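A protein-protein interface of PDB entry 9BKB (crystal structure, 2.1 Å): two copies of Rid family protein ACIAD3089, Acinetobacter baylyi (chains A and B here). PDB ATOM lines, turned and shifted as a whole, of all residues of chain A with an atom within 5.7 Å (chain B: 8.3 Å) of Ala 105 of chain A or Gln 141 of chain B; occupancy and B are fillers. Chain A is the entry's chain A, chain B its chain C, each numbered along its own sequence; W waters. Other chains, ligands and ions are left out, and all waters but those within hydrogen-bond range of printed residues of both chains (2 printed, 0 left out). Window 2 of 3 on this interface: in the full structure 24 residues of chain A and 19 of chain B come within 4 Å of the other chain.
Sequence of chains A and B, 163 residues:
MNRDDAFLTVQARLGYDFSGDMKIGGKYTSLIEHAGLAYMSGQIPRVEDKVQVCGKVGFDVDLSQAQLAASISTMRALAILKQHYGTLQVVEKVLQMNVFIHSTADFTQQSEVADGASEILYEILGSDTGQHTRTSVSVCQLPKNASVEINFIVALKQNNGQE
Of the printed residues of chain B, Thr 104 of chain A touches Gln 141 (3.9 Å).
Of chain B, only Cys 140 (3.9 Å) and Gln 141 (3.0 Å) come within 4 Å of Ala 105 of chain A.
Asp 106 of chain A touches none of the printed residues of chain B.
Of the printed residues of chain B, Phe 107 of chain A touches Gln 141.
Of the printed residues of chain B, Gln 110 of chain A touches Gln 141 (3.5 Å), Leu 142 (3.4 Å) and Pro 143 (3.3 Å).
Of the printed residues of chain A, Phe 100 of chain B touches Val 137.
Ser 138 of chain B touches none of the printed residues of chain A.
The nearest residue of chain A that does not touch Gln 141 of chain B is Asp 106 of chain A (4.1 Å).
The nearest printed residue of chain B that does not touch Val 139 of chain A is Val 139 of chain B (5.1 Å).
Printed residues of chain B that touch a printed residue of chain A: Phe 100, Val 139, Cys 140, Gln 141, Leu 142, Pro 143, Lys 144, Asn 145 and Glu 149.
Printed residues of chain A that touch a printed residue of chain B: Ser 103, Thr 104, Ala 105, Phe 107, Thr 108, Gln 110, Val 137, Ser 138 and Val 139.
Hydrophobic or aromatic side chains of chain A that line the printed part of chain B: Val 137.
Along chain A the printed residues that touch a printed residue of chain B span positions 103 to 139.
Among the printed residues, no Asp or Glu carboxylate lies within 4 Å of a Lys or Arg side-chain nitrogen of the other chain.
O of Ser 103 of chain A is in hydrogen-bond range of SG of Cys 140 of chain B (3.7 Å).
NE2 of Gln 141 of chain B sits at hydrogen-bond distance from O of Ala 105 of chain A, 3.0 Å away.
O of Thr 108 of chain A lies within hydrogen-bond range of N of Lys 144 of chain B (3.2 Å).
The side-chain amide oxygen of Gln 110 of chain A sits close to the backbone carbonyl oxygen of Leu 142 of chain B, at 3.4 Å.
The backbone carbonyl oxygen (O) of Ser 138 of chain A lies within hydrogen-bond range of the backbone NH (N) of Cys 140 of chain B, at 3.3 Å.
N of Ser 138 of chain A sits at hydrogen-bond distance from O of Gln 141 of chain B.
The backbone carbonyl oxygen (O) of Val 139 of chain A is in hydrogen-bond range of the side-chain sulfur (SG) of Cys 140 of chain B (3.5 Å).
The side-chain amide oxygen (OE1) of Gln 110 of chain A sits close to the backbone nitrogen (N) of Pro 143 of chain B (3.3 Å).
Ser 138 of chain A touches Val 139 of chain B, but with the chains exchanged Val 139 of chain A does not touch Ser 138 of chain B (6.6 Å).
3 positions are printed for both chains.
The side-chain hydroxyl (OG) of Ser 103 of chain A lies within hydrogen-bond range of the side-chain hydroxyl (OG) of Ser 138 of chain A (2.7 Å).
The side-chain sulfur (SG) of Cys 54 of chain B sits at hydrogen-bond distance from the backbone carbonyl oxygen (O) of Lys 144 of chain B.
N of Phe 100 of chain B is in hydrogen-bond range of O of Glu 149 of chain B (2.8 Å).
ND1 of His 102 of chain B sits close to O of Cys 140 of chain B (3.4 Å).
The side-chain amide oxygen of Gln 141 of chain B sits close to a ring nitrogen (NE2) of His 102 of chain B (3.3 Å).
The side-chain amide nitrogen (NE2) of Gln 141 of chain B is in hydrogen-bond range of the side-chain amide oxygen (OD1) of Asn 145 of chain B (2.9 Å).
Water W1 lies within hydrogen-bond range of the backbone carbonyl oxygen (O) of Ala 105 of chain A, a ring nitrogen (NE2) of His 102 of chain B and the side-chain amide nitrogen (NE2) of Gln 141 of chain B.
Water W2 lies within hydrogen-bond range of the backbone carbonyl oxygen of Thr 108 of chain A (2.9 Å), the side-chain amino group of Lys 144 of chain B (3.1 Å) and the backbone NH of Gln 110 of chain A (3.3 Å).
Among the printed residues, pairs that only touch across the chains: Thr 104 of chain A with Gln 141 of chain B, Ala 105 of chain A with Cys 140 of chain B, Phe 107 of chain A with Gln 141 of chain B, Thr 108 of chain A with Gln 141 of chain B, Thr 108 of chain A with Pro 143 of chain B, Thr 108 of chain A with Asn 145 of chain B, Gln 110 of chain A with Gln 141 of chain B, Val 137 of chain A with Phe 100 of chain B, Val 137 of chain A with Leu 142 of chain B, Val 137 of chain A with Glu 149 of chain B and Ser 138 of chain A with Val 139 of chain B.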
ATOM      1  N   SER A 103      21.950   4.348  -9.503  1.00  0.00           N
ATOM      2  CA  SER A 103      21.843   3.121  -8.713  1.00  0.00           C
ATOM      3  C   SER A 103      20.775   3.228  -7.623  1.00  0.00           C
ATOM      4  O   SER A 103      20.188   4.285  -7.377  1.00  0.00           O
ATOM      5  CB  SER A 103      23.175   2.751  -8.051  1.00  0.00           C
ATOM      6  OG  SER A 103      23.343   3.445  -6.815  1.00  0.00           O
ATOM      7  N   THR A 104      20.539   2.096  -6.960  1.00  0.00           N
ATOM      8  CA  THR A 104      19.677   2.014  -5.791  1.00  0.00           C
ATOM      9  C   THR A 104      20.396   2.546  -4.549  1.00  0.00           C
ATOM     10  O   THR A 104      21.621   2.697  -4.516  1.00  0.00           O
ATOM     11  CB  THR A 104      19.273   0.569  -5.532  1.00  0.00           C
ATOM     12  OG1 THR A 104      20.450  -0.173  -5.203  1.00  0.00           O
ATOM     13  CG2 THR A 104      18.634  -0.048  -6.769  1.00  0.00           C
ATOM     14  N   ALA A 105      19.623   2.766  -3.491  1.00  0.00           N
ATOM     15  CA  ALA A 105      20.168   3.277  -2.240  1.00  0.00           C
ATOM     16  C   ALA A 105      20.877   2.208  -1.432  1.00  0.00           C
ATOM     17  O   ALA A 105      21.347   2.503  -0.326  1.00  0.00           O
ATOM     18  CB  ALA A 105      19.057   3.902  -1.383  1.00  0.00           C
ATOM     19  N   ASP A 106      20.962   0.982  -1.950  1.00  0.00           N
ATOM     20  CA  ASP A 106      21.708  -0.078  -1.289  1.00  0.00           C
ATOM     21  C   ASP A 106      22.938  -0.507  -2.066  1.00  0.00           C
ATOM     22  O   ASP A 106      23.658  -1.398  -1.614  1.00  0.00           O
ATOM     23  CB  ASP A 106      20.809  -1.299  -1.067  1.00  0.00           C
ATOM     24  CG  ASP A 106      19.463  -0.928  -0.481  1.00  0.00           C
ATOM     25  OD1 ASP A 106      19.438  -0.229   0.564  1.00  0.00           O
ATOM     26  OD2 ASP A 106      18.430  -1.317  -1.078  1.00  0.00           O
ATOM     27  N   PHE A 107      23.214   0.115  -3.205  1.00  0.00           N
ATOM     28  CA  PHE A 107      24.379  -0.243  -3.999  1.00  0.00           C
ATOM     29  C   PHE A 107      25.636   0.367  -3.392  1.00  0.00           C
ATOM     30  O   PHE A 107      25.682   1.566  -3.112  1.00  0.00           O
ATOM     31  CB  PHE A 107      24.184   0.234  -5.436  1.00  0.00           C
ATOM     32  CG  PHE A 107      25.232  -0.262  -6.381  1.00  0.00           C
ATOM     33  CD1 PHE A 107      25.249  -1.592  -6.782  1.00  0.00           C
ATOM     34  CD2 PHE A 107      26.207   0.589  -6.861  1.00  0.00           C
ATOM     35  CE1 PHE A 107      26.223  -2.052  -7.657  1.00  0.00           C
ATOM     36  CE2 PHE A 107      27.178   0.133  -7.735  1.00  0.00           C
ATOM     37  CZ  PHE A 107      27.187  -1.187  -8.126  1.00  0.00           C
ATOM     38  N   THR A 108      26.660  -0.460  -3.168  1.00  0.00           N
ATOM     39  CA  THR A 108      27.902   0.032  -2.585  1.00  0.00           C
ATOM     40  C   THR A 108      29.136  -0.376  -3.382  1.00  0.00           C
ATOM     41  O   THR A 108      30.255  -0.244  -2.874  1.00  0.00           O
ATOM     42  CB  THR A 108      28.064  -0.441  -1.135  1.00  0.00           C
ATOM     43  OG1 THR A 108      28.118  -1.867  -1.105  1.00  0.00           O
ATOM     44  CG2 THR A 108      26.894   0.038  -0.270  1.00  0.00           C
ATOM     45  N   GLN A 110      30.394   0.991  -6.224  1.00  0.00           N
ATOM     46  CA  GLN A 110      30.703   2.019  -7.215  1.00  0.00           C
ATOM     47  C   GLN A 110      32.129   1.877  -7.726  1.00  0.00           C
ATOM     48  O   GLN A 110      32.404   2.115  -8.910  1.00  0.00           O
ATOM     49  CB  GLN A 110      30.498   3.409  -6.604  1.00  0.00           C
ATOM     50  CG  GLN A 110      29.032   3.738  -6.264  1.00  0.00           C
ATOM     51  CD  GLN A 110      28.586   3.145  -4.936  1.00  0.00           C
ATOM     52  OE1 GLN A 110      29.331   2.405  -4.282  1.00  0.00           O
ATOM     53  NE2 GLN A 110      27.372   3.486  -4.518  1.00  0.00           N
ATOM     54  N   VAL A 137      30.506   8.004  -7.653  1.00  0.00           N
ATOM     55  CA  VAL A 137      29.388   8.204  -6.742  1.00  0.00           C
ATOM     56  C   VAL A 137      28.116   7.699  -7.409  1.00  0.00           C
ATOM     57  O   VAL A 137      28.027   7.598  -8.633  1.00  0.00           O
ATOM     58  CB  VAL A 137      29.198   9.675  -6.320  1.00  0.00           C
ATOM     59  CG1 VAL A 137      30.500  10.265  -5.749  1.00  0.00           C
ATOM     60  CG2 VAL A 137      28.665  10.500  -7.493  1.00  0.00           C
ATOM     61  N   SER A 138      27.126   7.385  -6.575  1.00  0.00           N
ATOM     62  CA  SER A 138      25.802   6.997  -7.052  1.00  0.00           C
ATOM     63  C   SER A 138      24.921   8.229  -7.136  1.00  0.00           C
ATOM     64  O   SER A 138      24.879   9.030  -6.199  1.00  0.00           O
ATOM     65  CB  SER A 138      25.150   5.973  -6.120  1.00  0.00           C
ATOM     66  OG  SER A 138      25.695   4.675  -6.325  1.00  0.00           O
ATOM     67  N   VAL A 139      24.207   8.368  -8.253  1.00  0.00           N
ATOM     68  CA  VAL A 139      23.215   9.412  -8.430  1.00  0.00           C
ATOM     69  C   VAL A 139      21.854   8.736  -8.561  1.00  0.00           C
ATOM     70  O   VAL A 139      21.751   7.524  -8.742  1.00  0.00           O
ATOM     71  CB  VAL A 139      23.497  10.302  -9.650  1.00  0.00           C
ATOM     72  CG1 VAL A 139      24.830  11.031  -9.476  1.00  0.00           C
ATOM     73  CG2 VAL A 139      23.475   9.469 -10.918  1.00  0.00           C
ATOM     74  N   CYS B  54      30.029   5.330   8.363  1.00  0.00           N
ATOM     75  CA  CYS B  54      29.213   4.837   7.264  1.00  0.00           C
ATOM     76  C   CYS B  54      27.739   5.022   7.564  1.00  0.00           C
ATOM     77  O   CYS B  54      27.321   5.040   8.723  1.00  0.00           O
ATOM     78  CB  CYS B  54      29.511   3.369   6.983  1.00  0.00           C
ATOM     79  SG  CYS B  54      31.164   3.146   6.334  1.00  0.00           S
ATOM     80  N   GLY B  55      26.958   5.186   6.504  1.00  0.00           N
ATOM     81  CA  GLY B  55      25.523   5.313   6.602  1.00  0.00           C
ATOM     82  C   GLY B  55      25.021   6.538   5.871  1.00  0.00           C
ATOM     83  O   GLY B  55      25.761   7.250   5.199  1.00  0.00           O
ATOM     84  N   LYS B  56      23.716   6.765   6.010  1.00  0.00           N
ATOM     85  CA  LYS B  56      22.993   7.790   5.270  1.00  0.00           C
ATOM     86  C   LYS B  56      22.723   8.965   6.200  1.00  0.00           C
ATOM     87  O   LYS B  56      22.066   8.805   7.237  1.00  0.00           O
ATOM     88  CB  LYS B  56      21.691   7.206   4.704  1.00  0.00           C
ATOM     89  CG  LYS B  56      20.825   8.161   3.899  1.00  0.00           C
ATOM     90  CD  LYS B  56      19.749   7.424   3.067  1.00  0.00           C
ATOM     91  CE  LYS B  56      18.826   6.551   3.920  1.00  0.00           C
ATOM     92  NZ  LYS B  56      17.844   5.807   3.048  1.00  0.00           N
ATOM     93  N   PHE B 100      30.522  15.223  -1.741  1.00  0.00           N
ATOM     94  CA  PHE B 100      29.363  14.398  -2.066  1.00  0.00           C
ATOM     95  C   PHE B 100      28.878  13.730  -0.786  1.00  0.00           C
ATOM     96  O   PHE B 100      29.629  12.983  -0.150  1.00  0.00           O
ATOM     97  CB  PHE B 100      29.713  13.354  -3.132  1.00  0.00           C
ATOM     98  CG  PHE B 100      30.229  13.965  -4.419  1.00  0.00           C
ATOM     99  CD1 PHE B 100      29.348  14.394  -5.392  1.00  0.00           C
ATOM    100  CD2 PHE B 100      31.588  14.144  -4.633  1.00  0.00           C
ATOM    101  CE1 PHE B 100      29.810  14.973  -6.568  1.00  0.00           C
ATOM    102  CE2 PHE B 100      32.064  14.737  -5.814  1.00  0.00           C
ATOM    103  CZ  PHE B 100      31.188  15.144  -6.769  1.00  0.00           C
ATOM    104  N   ILE B 101      27.622  13.988  -0.421  1.00  0.00           N
ATOM    105  CA  ILE B 101      27.059  13.541   0.847  1.00  0.00           C
ATOM    106  C   ILE B 101      25.963  12.518   0.577  1.00  0.00           C
ATOM    107  O   ILE B 101      24.982  12.806  -0.118  1.00  0.00           O
ATOM    108  CB  ILE B 101      26.507  14.716   1.659  1.00  0.00           C
ATOM    109  CG1 ILE B 101      27.596  15.773   1.836  1.00  0.00           C
ATOM    110  CG2 ILE B 101      26.012  14.202   3.027  1.00  0.00           C
ATOM    111  CD1 ILE B 101      27.048  17.126   2.162  1.00  0.00           C
ATOM    112  N   HIS B 102      26.134  11.332   1.143  1.00  0.00           N
ATOM    113  CA  HIS B 102      25.175  10.230   1.133  1.00  0.00           C
ATOM    114  C   HIS B 102      24.077  10.574   2.151  1.00  0.00           C
ATOM    115  O   HIS B 102      24.297  10.504   3.361  1.00  0.00           O
ATOM    116  CB  HIS B 102      25.950   8.960   1.481  1.00  0.00           C
ATOM    117  CG  HIS B 102      25.138   7.712   1.596  1.00  0.00           C
ATOM    118  ND1 HIS B 102      23.812   7.627   1.220  1.00  0.00           N
ATOM    119  CD2 HIS B 102      25.484   6.480   2.039  1.00  0.00           C
ATOM    120  CE1 HIS B 102      23.379   6.400   1.433  1.00  0.00           C
ATOM    121  NE2 HIS B 102      24.370   5.685   1.933  1.00  0.00           N
ATOM    122  N   SER B 103      22.895  10.991   1.683  1.00  0.00           N
ATOM    123  CA  SER B 103      21.882  11.515   2.600  1.00  0.00           C
ATOM    124  C   SER B 103      20.479  11.075   2.188  1.00  0.00           C
ATOM    125  O   SER B 103      20.267  10.447   1.145  1.00  0.00           O
ATOM    126  CB  SER B 103      21.913  13.053   2.684  1.00  0.00           C
ATOM    127  OG  SER B 103      21.167  13.642   1.617  1.00  0.00           O
ATOM    128  N   SER B 138      24.002  16.231  -2.299  1.00  0.00           N
ATOM    129  CA  SER B 138      23.615  14.946  -1.741  1.00  0.00           C
ATOM    130  C   SER B 138      23.575  13.908  -2.850  1.00  0.00           C
ATOM    131  O   SER B 138      23.029  14.166  -3.924  1.00  0.00           O
ATOM    132  CB  SER B 138      22.245  15.031  -1.060  1.00  0.00           C
ATOM    133  OG  SER B 138      22.342  15.644   0.208  1.00  0.00           O
ATOM    134  N   VAL B 139      24.160  12.740  -2.593  1.00  0.00           N
ATOM    135  CA  VAL B 139      24.091  11.617  -3.516  1.00  0.00           C
ATOM    136  C   VAL B 139      23.335  10.496  -2.810  1.00  0.00           C
ATOM    137  O   VAL B 139      23.179  10.502  -1.592  1.00  0.00           O
ATOM    138  CB  VAL B 139      25.488  11.139  -3.969  1.00  0.00           C
ATOM    139  CG1 VAL B 139      26.230  12.254  -4.725  1.00  0.00           C
ATOM    140  CG2 VAL B 139      26.305  10.653  -2.783  1.00  0.00           C
ATOM    141  N   CYS B 140      22.899   9.503  -3.576  1.00  0.00           N
ATOM    142  CA  CYS B 140      22.084   8.482  -2.935  1.00  0.00           C
ATOM    143  C   CYS B 140      22.882   7.287  -2.421  1.00  0.00           C
ATOM    144  O   CYS B 140      22.328   6.498  -1.652  1.00  0.00           O
ATOM    145  CB  CYS B 140      20.975   8.017  -3.886  1.00  0.00           C
ATOM    146  SG  CYS B 140      21.496   7.029  -5.276  1.00  0.00           S
ATOM    147  N   GLN B 141      24.165   7.157  -2.773  1.00  0.00           N
ATOM    148  CA  GLN B 141      25.040   6.141  -2.187  1.00  0.00           C
ATOM    149  C   GLN B 141      26.489   6.454  -2.543  1.00  0.00           C
ATOM    150  O   GLN B 141      26.773   7.228  -3.462  1.00  0.00           O
ATOM    151  CB  GLN B 141      24.682   4.717  -2.650  1.00  0.00           C
ATOM    152  CG  GLN B 141      23.953   3.857  -1.588  1.00  0.00           C
ATOM    153  CD  GLN B 141      24.817   3.464  -0.390  1.00  0.00           C
ATOM    154  OE1 GLN B 141      25.962   3.890  -0.262  1.00  0.00           O
ATOM    155  NE2 GLN B 141      24.257   2.646   0.504  1.00  0.00           N
ATOM    156  N   LEU B 142      27.399   5.821  -1.818  1.00  0.00           N
ATOM    157  CA  LEU B 142      28.830   6.012  -1.976  1.00  0.00           C
ATOM    158  C   LEU B 142      29.534   4.678  -1.800  1.00  0.00           C
ATOM    159  O   LEU B 142      28.957   3.743  -1.227  1.00  0.00           O
ATOM    160  CB  LEU B 142      29.388   7.007  -0.949  1.00  0.00           C
ATOM    161  CG  LEU B 142      29.012   8.448  -1.193  1.00  0.00           C
ATOM    162  CD1 LEU B 142      29.509   9.308  -0.034  1.00  0.00           C
ATOM    163  CD2 LEU B 142      29.585   8.918  -2.543  1.00  0.00           C
ATOM    164  N   PRO B 143      30.774   4.555  -2.293  1.00  0.00           N
ATOM    165  CA  PRO B 143      31.542   3.325  -2.078  1.00  0.00           C
ATOM    166  C   PRO B 143      31.502   2.900  -0.625  1.00  0.00           C
ATOM    167  O   PRO B 143      31.664   3.719   0.284  1.00  0.00           O
ATOM    168  CB  PRO B 143      32.965   3.708  -2.507  1.00  0.00           C
ATOM    169  CG  PRO B 143      32.766   4.755  -3.559  1.00  0.00           C
ATOM    170  CD  PRO B 143      31.477   5.491  -3.201  1.00  0.00           C
ATOM    171  N   LYS B 144      31.274   1.602  -0.417  1.00  0.00           N
ATOM    172  CA  LYS B 144      31.300   0.977   0.907  1.00  0.00           C
ATOM    173  C   LYS B 144      30.336   1.643   1.884  1.00  0.00           C
ATOM    174  O   LYS B 144      30.606   1.697   3.082  1.00  0.00           O
ATOM    175  CB  LYS B 144      32.712   0.978   1.500  1.00  0.00           C
ATOM    176  CG  LYS B 144      33.824   0.774   0.485  1.00  0.00           C
ATOM    177  CD  LYS B 144      33.971  -0.672   0.061  1.00  0.00           C
ATOM    178  CE  LYS B 144      35.230  -0.830  -0.801  1.00  0.00           C
ATOM    179  NZ  LYS B 144      35.151  -0.052  -2.099  1.00  0.00           N
ATOM    180  N   ASN B 145      29.212   2.162   1.383  1.00  0.00           N
ATOM    181  CA  ASN B 145      28.172   2.776   2.212  1.00  0.00           C
ATOM    182  C   ASN B 145      28.681   4.018   2.957  1.00  0.00           C
ATOM    183  O   ASN B 145      28.076   4.447   3.947  1.00  0.00           O
ATOM    184  CB  ASN B 145      27.592   1.750   3.204  1.00  0.00           C
ATOM    185  CG  ASN B 145      26.295   2.212   3.834  1.00  0.00           C
ATOM    186  OD1 ASN B 145      25.455   2.812   3.175  1.00  0.00           O
ATOM    187  ND2 ASN B 145      26.140   1.956   5.124  1.00  0.00           N
ATOM    188  N   ALA B 146      29.766   4.632   2.479  1.00  0.00           N
ATOM    189  CA  ALA B 146      30.326   5.799   3.143  1.00  0.00           C
ATOM    190  C   ALA B 146      29.306   6.932   3.202  1.00  0.00           C
ATOM    191  O   ALA B 146      28.384   7.018   2.387  1.00  0.00           O
ATOM    192  CB  ALA B 146      31.590   6.267   2.408  1.00  0.00           C
ATOM    193  N   SER B 147      29.475   7.811   4.181  1.00  0.00           N
ATOM    194  CA  SER B 147      28.550   8.926   4.321  1.00  0.00           C
ATOM    195  C   SER B 147      28.993  10.161   3.548  1.00  0.00           C
ATOM    196  O   SER B 147      28.140  10.975   3.174  1.00  0.00           O
ATOM    197  CB  SER B 147      28.372   9.286   5.798  1.00  0.00           C
ATOM    198  OG  SER B 147      29.627   9.622   6.358  1.00  0.00           O
ATOM    199  N   VAL B 148      30.302  10.337   3.318  1.00  0.00           N
ATOM    200  CA  VAL B 148      30.832  11.484   2.588  1.00  0.00           C
ATOM    201  C   VAL B 148      31.995  11.032   1.709  1.00  0.00           C
ATOM    202  O   VAL B 148      32.761  10.128   2.069  1.00  0.00           O
ATOM    203  CB  VAL B 148      31.296  12.618   3.540  1.00  0.00           C
ATOM    204  CG1 VAL B 148      31.688  13.857   2.744  1.00  0.00           C
ATOM    205  CG2 VAL B 148      30.203  12.975   4.547  1.00  0.00           C
ATOM    206  N   GLU B 149      32.122  11.668   0.542  1.00  0.00           N
ATOM    207  CA  GLU B 149      33.286  11.516  -0.328  1.00  0.00           C
ATOM    208  C   GLU B 149      33.709  12.886  -0.835  1.00  0.00           C
ATOM    209  O   GLU B 149      32.864  13.676  -1.260  1.00  0.00           O
ATOM    210  CB  GLU B 149      32.984  10.589  -1.514  1.00  0.00           C
ATOM    211  CG  GLU B 149      34.210  10.267  -2.406  1.00  0.00           C
ATOM    212  CD  GLU B 149      33.889   9.292  -3.540  1.00  0.00           C
ATOM    213  OE1 GLU B 149      34.518   9.401  -4.614  1.00  0.00           O
ATOM    214  OE2 GLU B 149      32.951   8.478  -3.406  1.00  0.00           O
HETATM  215  O   HOH W   1      21.385   4.358   1.486  1.00  0.00           O
HETATM  216  O   HOH W   2      32.781   0.523  -4.006  1.00  0.00           O
